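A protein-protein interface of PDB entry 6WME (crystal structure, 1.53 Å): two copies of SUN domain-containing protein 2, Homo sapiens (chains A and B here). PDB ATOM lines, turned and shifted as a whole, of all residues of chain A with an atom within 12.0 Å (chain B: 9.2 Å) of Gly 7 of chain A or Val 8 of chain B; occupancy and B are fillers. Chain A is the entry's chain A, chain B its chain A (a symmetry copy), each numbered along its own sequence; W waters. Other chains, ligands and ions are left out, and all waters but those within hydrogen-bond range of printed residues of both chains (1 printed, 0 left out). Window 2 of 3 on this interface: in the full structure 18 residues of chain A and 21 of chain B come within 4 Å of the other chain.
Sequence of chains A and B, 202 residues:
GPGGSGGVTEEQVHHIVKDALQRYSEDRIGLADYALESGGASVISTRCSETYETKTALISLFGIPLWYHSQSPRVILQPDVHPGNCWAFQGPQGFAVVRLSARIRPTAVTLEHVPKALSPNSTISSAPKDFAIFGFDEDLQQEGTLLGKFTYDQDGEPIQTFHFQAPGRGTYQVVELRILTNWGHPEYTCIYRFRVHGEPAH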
ATOM      1  N   GLY A   7     -14.601  25.613   4.617  1.00  0.00           N
ATOM      2  CA  GLY A   7     -16.013  25.728   4.945  1.00  0.00           C
ATOM      3  C   GLY A   7     -16.707  24.381   4.947  1.00  0.00           C
ATOM      4  O   GLY A   7     -16.072  23.350   5.157  1.00  0.00           O
ATOM      5  N   VAL A   8     -18.016  24.380   4.713  1.00  0.00           N
ATOM      6  CA  VAL A   8     -18.798  23.152   4.706  1.00  0.00           C
ATOM      7  C   VAL A   8     -19.274  22.900   3.285  1.00  0.00           C
ATOM      8  O   VAL A   8     -19.442  23.835   2.494  1.00  0.00           O
ATOM      9  CB  VAL A   8     -19.992  23.241   5.678  1.00  0.00           C
ATOM     10  CG1 VAL A   8     -19.516  23.721   7.041  1.00  0.00           C
ATOM     11  CG2 VAL A   8     -21.074  24.143   5.115  1.00  0.00           C
ATOM     12  N   THR A   9     -19.501  21.633   2.960  1.00  0.00           N
ATOM     13  CA  THR A   9     -20.047  21.303   1.653  1.00  0.00           C
ATOM     14  C   THR A   9     -21.576  21.302   1.691  1.00  0.00           C
ATOM     15  O   THR A   9     -22.197  21.276   2.760  1.00  0.00           O
ATOM     16  CB  THR A   9     -19.534  19.948   1.168  1.00  0.00           C
ATOM     17  OG1 THR A   9     -20.057  18.903   1.995  1.00  0.00           O
ATOM     18  CG2 THR A   9     -17.997  19.906   1.197  1.00  0.00           C
ATOM     19  N   GLU A  10     -22.182  21.337   0.497  1.00  0.00           N
ATOM     20  CA  GLU A  10     -23.641  21.264   0.404  1.00  0.00           C
ATOM     21  C   GLU A  10     -24.174  19.955   0.986  1.00  0.00           C
ATOM     22  O   GLU A  10     -25.181  19.948   1.707  1.00  0.00           O
ATOM     23  CB  GLU A  10     -24.079  21.432  -1.057  1.00  0.00           C
ATOM     24  CG  GLU A  10     -25.550  21.105  -1.311  1.00  0.00           C
ATOM     25  CD  GLU A  10     -25.932  21.194  -2.776  1.00  0.00           C
ATOM     26  OE1 GLU A  10     -27.117  20.962  -3.095  1.00  0.00           O
ATOM     27  OE2 GLU A  10     -25.051  21.494  -3.611  1.00  0.00           O
ATOM     28  N   GLU A  11     -23.498  18.840   0.712  1.00  0.00           N
ATOM     29  CA  GLU A  11     -23.952  17.555   1.243  1.00  0.00           C
ATOM     30  C   GLU A  11     -23.904  17.552   2.766  1.00  0.00           C
ATOM     31  O   GLU A  11     -24.811  17.029   3.429  1.00  0.00           O
ATOM     32  CB  GLU A  11     -23.092  16.429   0.670  1.00  0.00           C
ATOM     33  CG  GLU A  11     -23.536  15.041   1.077  1.00  0.00           C
ATOM     34  CD  GLU A  11     -22.795  13.956   0.319  1.00  0.00           C
ATOM     35  OE1 GLU A  11     -22.093  13.149   0.964  1.00  0.00           O
ATOM     36  OE2 GLU A  11     -22.912  13.909  -0.924  1.00  0.00           O
ATOM     37  N   GLN A  12     -22.872  18.178   3.336  1.00  0.00           N
ATOM     38  CA  GLN A  12     -22.752  18.285   4.787  1.00  0.00           C
ATOM     39  C   GLN A  12     -23.885  19.110   5.391  1.00  0.00           C
ATOM     40  O   GLN A  12     -24.422  18.758   6.456  1.00  0.00           O
ATOM     41  CB  GLN A  12     -21.399  18.897   5.138  1.00  0.00           C
ATOM     42  CG  GLN A  12     -21.044  18.859   6.603  1.00  0.00           C
ATOM     43  CD  GLN A  12     -19.620  19.312   6.846  1.00  0.00           C
ATOM     44  OE1 GLN A  12     -18.845  19.500   5.902  1.00  0.00           O
ATOM     45  NE2 GLN A  12     -19.262  19.483   8.115  1.00  0.00           N
ATOM     46  N   VAL A  13     -24.264  20.215   4.743  1.00  0.00           N
ATOM     47  CA  VAL A  13     -25.384  21.009   5.262  1.00  0.00           C
ATOM     48  C   VAL A  13     -26.664  20.173   5.284  1.00  0.00           C
ATOM     49  O   VAL A  13     -27.413  20.177   6.274  1.00  0.00           O
ATOM     50  CB  VAL A  13     -25.558  22.301   4.436  1.00  0.00           C
ATOM     51  CG1 VAL A  13     -26.797  23.057   4.878  1.00  0.00           C
ATOM     52  CG2 VAL A  13     -24.345  23.199   4.582  1.00  0.00           C
ATOM     53  N   HIS A  14     -26.916  19.415   4.212  1.00  0.00           N
ATOM     54  CA  HIS A  14     -28.128  18.598   4.157  1.00  0.00           C
ATOM     55  C   HIS A  14     -28.134  17.537   5.253  1.00  0.00           C
ATOM     56  O   HIS A  14     -29.181  17.256   5.845  1.00  0.00           O
ATOM     57  CB  HIS A  14     -28.277  17.962   2.771  1.00  0.00           C
ATOM     58  CG  HIS A  14     -28.886  18.891   1.765  1.00  0.00           C
ATOM     59  ND1 HIS A  14     -30.249  19.075   1.656  1.00  0.00           N
ATOM     60  CD2 HIS A  14     -28.322  19.721   0.857  1.00  0.00           C
ATOM     61  CE1 HIS A  14     -30.498  19.959   0.706  1.00  0.00           C
ATOM     62  NE2 HIS A  14     -29.346  20.365   0.203  1.00  0.00           N
ATOM     63  N   HIS A  15     -26.972  16.952   5.552  1.00  0.00           N
ATOM     64  CA  HIS A  15     -26.910  15.964   6.626  1.00  0.00           C
ATOM     65  C   HIS A  15     -27.222  16.597   7.981  1.00  0.00           C
ATOM     66  O   HIS A  15     -27.970  16.027   8.789  1.00  0.00           O
ATOM     67  CB  HIS A  15     -25.531  15.299   6.633  1.00  0.00           C
ATOM     68  CG  HIS A  15     -25.420  14.137   7.569  1.00  0.00           C
ATOM     69  ND1 HIS A  15     -25.889  12.880   7.252  1.00  0.00           N
ATOM     70  CD2 HIS A  15     -24.888  14.039   8.810  1.00  0.00           C
ATOM     71  CE1 HIS A  15     -25.653  12.058   8.258  1.00  0.00           C
ATOM     72  NE2 HIS A  15     -25.047  12.735   9.217  1.00  0.00           N
ATOM     73  N   ILE A  16     -26.673  17.784   8.242  1.00  0.00           N
ATOM     74  CA  ILE A  16     -26.931  18.487   9.494  1.00  0.00           C
ATOM     75  C   ILE A  16     -28.420  18.775   9.656  1.00  0.00           C
ATOM     76  O   ILE A  16     -29.003  18.557  10.731  1.00  0.00           O
ATOM     77  CB  ILE A  16     -26.097  19.783   9.539  1.00  0.00           C
ATOM     78  CG1 ILE A  16     -24.622  19.447   9.765  1.00  0.00           C
ATOM     79  CG2 ILE A  16     -26.592  20.705  10.638  1.00  0.00           C
ATOM     80  CD1 ILE A  16     -23.708  20.588   9.437  1.00  0.00           C
ATOM     81  N   VAL A  17     -29.059  19.264   8.594  1.00  0.00           N
ATOM     82  CA  VAL A  17     -30.489  19.569   8.643  1.00  0.00           C
ATOM     83  C   VAL A  17     -31.308  18.291   8.837  1.00  0.00           C
ATOM     84  O   VAL A  17     -32.248  18.252   9.648  1.00  0.00           O
ATOM     85  CB  VAL A  17     -30.882  20.327   7.360  1.00  0.00           C
ATOM     86  CG1 VAL A  17     -32.385  20.440   7.242  1.00  0.00           C
ATOM     87  CG2 VAL A  17     -30.220  21.702   7.320  1.00  0.00           C
ATOM     88  N   GLY B   7     -16.873  30.927   2.771  1.00  0.00           N
ATOM     89  CA  GLY B   7     -18.081  30.152   3.002  1.00  0.00           C
ATOM     90  C   GLY B   7     -18.549  30.243   4.439  1.00  0.00           C
ATOM     91  O   GLY B   7     -18.259  31.218   5.131  1.00  0.00           O
ATOM     92  N   VAL B   8     -19.276  29.230   4.900  1.00  0.00           N
ATOM     93  CA  VAL B   8     -19.798  29.211   6.260  1.00  0.00           C
ATOM     94  C   VAL B   8     -19.089  28.107   7.026  1.00  0.00           C
ATOM     95  O   VAL B   8     -18.634  27.117   6.441  1.00  0.00           O
ATOM     96  CB  VAL B   8     -21.325  28.994   6.271  1.00  0.00           C
ATOM     97  CG1 VAL B   8     -21.995  29.967   5.312  1.00  0.00           C
ATOM     98  CG2 VAL B   8     -21.663  27.555   5.931  1.00  0.00           C
ATOM     99  N   THR B   9     -18.999  28.272   8.341  1.00  0.00           N
ATOM    100  CA  THR B   9     -18.419  27.225   9.167  1.00  0.00           C
ATOM    101  C   THR B   9     -19.495  26.236   9.620  1.00  0.00           C
ATOM    102  O   THR B   9     -20.699  26.506   9.535  1.00  0.00           O
ATOM    103  CB  THR B   9     -17.705  27.815  10.382  1.00  0.00           C
ATOM    104  OG1 THR B   9     -18.659  28.415  11.266  1.00  0.00           O
ATOM    105  CG2 THR B   9     -16.673  28.868   9.949  1.00  0.00           C
ATOM    106  N   GLU B  10     -19.042  25.071  10.100  1.00  0.00           N
ATOM    107  CA  GLU B  10     -19.973  24.076  10.635  1.00  0.00           C
ATOM    108  C   GLU B  10     -20.753  24.624  11.829  1.00  0.00           C
ATOM    109  O   GLU B  10     -21.969  24.412  11.941  1.00  0.00           O
ATOM    110  CB  GLU B  10     -19.210  22.801  11.016  1.00  0.00           C
ATOM    111  CG  GLU B  10     -20.031  21.800  11.830  1.00  0.00           C
ATOM    112  CD  GLU B  10     -19.228  20.593  12.269  1.00  0.00           C
ATOM    113  OE1 GLU B  10     -19.806  19.702  12.926  1.00  0.00           O
ATOM    114  OE2 GLU B  10     -18.018  20.530  11.959  1.00  0.00           O
ATOM    115  N   GLU B  11     -20.084  25.357  12.717  1.00  0.00           N
ATOM    116  CA  GLU B  11     -20.772  25.915  13.879  1.00  0.00           C
ATOM    117  C   GLU B  11     -21.849  26.904  13.447  1.00  0.00           C
ATOM    118  O   GLU B  11     -22.950  26.932  14.015  1.00  0.00           O
ATOM    119  CB  GLU B  11     -19.758  26.586  14.806  1.00  0.00           C
ATOM    120  CG  GLU B  11     -20.349  27.115  16.093  1.00  0.00           C
ATOM    121  CD  GLU B  11     -19.282  27.575  17.069  1.00  0.00           C
ATOM    122  OE1 GLU B  11     -19.265  28.775  17.415  1.00  0.00           O
ATOM    123  OE2 GLU B  11     -18.457  26.737  17.491  1.00  0.00           O
ATOM    124  N   GLN B  12     -21.560  27.689  12.408  1.00  0.00           N
ATOM    125  CA  GLN B  12     -22.535  28.635  11.873  1.00  0.00           C
ATOM    126  C   GLN B  12     -23.757  27.925  11.296  1.00  0.00           C
ATOM    127  O   GLN B  12     -24.898  28.382  11.485  1.00  0.00           O
ATOM    128  CB  GLN B  12     -21.867  29.500  10.809  1.00  0.00           C
ATOM    129  CG  GLN B  12     -22.690  30.670  10.332  1.00  0.00           C
ATOM    130  CD  GLN B  12     -21.895  31.581   9.421  1.00  0.00           C
ATOM    131  OE1 GLN B  12     -20.677  31.425   9.276  1.00  0.00           O
ATOM    132  NE2 GLN B  12     -22.574  32.544   8.806  1.00  0.00           N
ATOM    133  N   VAL B  13     -23.552  26.815  10.581  1.00  0.00           N
ATOM    134  CA  VAL B  13     -24.704  26.073  10.051  1.00  0.00           C
ATOM    135  C   VAL B  13     -25.590  25.582  11.195  1.00  0.00           C
ATOM    136  O   VAL B  13     -26.825  25.706  11.145  1.00  0.00           O
ATOM    137  CB  VAL B  13     -24.230  24.911   9.154  1.00  0.00           C
ATOM    138  CG1 VAL B  13     -25.407  24.059   8.715  1.00  0.00           C
ATOM    139  CG2 VAL B  13     -23.511  25.439   7.927  1.00  0.00           C
ATOM    140  N   HIS B  14     -24.978  25.053  12.259  1.00  0.00           N
ATOM    141  CA  HIS B  14     -25.764  24.550  13.386  1.00  0.00           C
ATOM    142  C   HIS B  14     -26.559  25.668  14.053  1.00  0.00           C
ATOM    143  O   HIS B  14     -27.705  25.461  14.463  1.00  0.00           O
ATOM    144  CB  HIS B  14     -24.852  23.842  14.394  1.00  0.00           C
ATOM    145  CG  HIS B  14     -24.543  22.427  14.009  1.00  0.00           C
ATOM    146  ND1 HIS B  14     -25.400  21.381  14.283  1.00  0.00           N
ATOM    147  CD2 HIS B  14     -23.501  21.891  13.331  1.00  0.00           C
ATOM    148  CE1 HIS B  14     -24.885  20.258  13.814  1.00  0.00           C
ATOM    149  NE2 HIS B  14     -23.732  20.540  13.234  1.00  0.00           N
ATOM    150  N   ILE B  16     -27.735  28.410  12.562  1.00  0.00           N
ATOM    151  CA  ILE B  16     -28.828  28.737  11.651  1.00  0.00           C
ATOM    152  C   ILE B  16     -29.969  27.734  11.795  1.00  0.00           C
ATOM    153  O   ILE B  16     -31.150  28.112  11.873  1.00  0.00           O
ATOM    154  CB  ILE B  16     -28.298  28.787  10.205  1.00  0.00           C
ATOM    155  CG1 ILE B  16     -27.449  30.044  10.004  1.00  0.00           C
ATOM    156  CG2 ILE B  16     -29.443  28.771   9.210  1.00  0.00           C
ATOM    157  CD1 ILE B  16     -26.591  29.976   8.777  1.00  0.00           C
HETATM  158  O   HOH W   1     -18.648  26.865   3.233  1.00  0.00           O
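Water W1 bridges N of Val 8 of chain A and N of Val 8 of chain B.
The backbone carbonyl oxygen (O) of Val 8 of chain B is in hydrogen-bond range of the backbone NH (N) of Val 8 of chain A, at 3.3 Å.
Of the 9 printed residues of chain B, 5 touch a printed residue of chain A.
Hydrophobic or aromatic side chains of chain B that line the printed part of chain A: Val 8, Val 13 and His 14.
Of the 11 printed residues of chain A, 3 touch a printed residue of chain B.
Hydrophobic or aromatic side chains of chain A within 4 Å of the printed part of chain B: Val 8 and Ile 16.
Along chain A the printed residues that touch a printed residue of chain B span positions 7 to 16.
Among the printed residues, no Asp or Glu carboxylate lies within 4 Å of a Lys or Arg side-chain nitrogen of the other chain.
Among the printed residues, pairs that only touch across the chains: Gly 7 of chain A with Val 8 of chain B (3.3 Å), Val 8 of chain A with Glu 10 of chain B (3.4 Å), Val 8 of chain A with Thr 9 of chain B (3.6 Å), Ile 16 of chain A with His 14 of chain B (3.6 Å), Ile 16 of chain A with Val 13 of chain B (3.9 Å) and Val 8 of chain A with Val 13 of chain B (3.9 Å).
Gly 7 of chain A touches Val 8 of chain B, but with the chains exchanged Val 8 of chain A does not touch Gly 7 of chain B (5.9 Å).
Val 8 of chain A touches its own counterpart, Val 8 of chain B.
Val 8 of chain A touches Thr 9 of chain B, but with the chains exchanged Thr 9 of chain A does not touch Val 8 of chain B (6.6 Å).
Ile 16 of chain A touches Val 13 of chain B, but with the chains exchanged Val 13 of chain A does not touch Ile 16 of chain B (7.6 Å).
OG1 of Thr 9 of chain B sits at hydrogen-bond distance from N of Gln 12 of chain B (3.2 Å).
Of the printed residues of chain B, Val 8 of chain A touches Val 8 (3.3 Å), Thr 9 (3.6 Å), Glu 10 (3.4 Å) and Val 13 (3.9 Å).
Gln 12 of chain A touches none of the printed residues of chain B.
His 14 of chain A touches none of the printed residues of chain B.
Of the printed residues of chain B, Ile 16 of chain A touches Val 13 (3.9 Å) and His 14 (3.6 Å).
No residue of chain A comes within 4 Å of Gly 7 of chain B.
Val 8 of chain B touches two residues of chain A.
Of chain A, only Val 8 comes within 4 Å of Thr 9 of chain B.
Printed residues of chain A within 4 Å of Glu 10 of chain B: Val 8.
No residue of chain A comes within 4 Å of Gln 12 of chain B.
Printed residues of chain A within 4 Å of His 14 of chain B: Ile 16.
The nearest residue of chain B that does not touch Gly 7 of chain A is Thr 9 of chain B (5.1 Å).
The nearest printed residue of chain B that does not touch Ile 16 of chain A is Glu 10 of chain B (4.6 Å).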
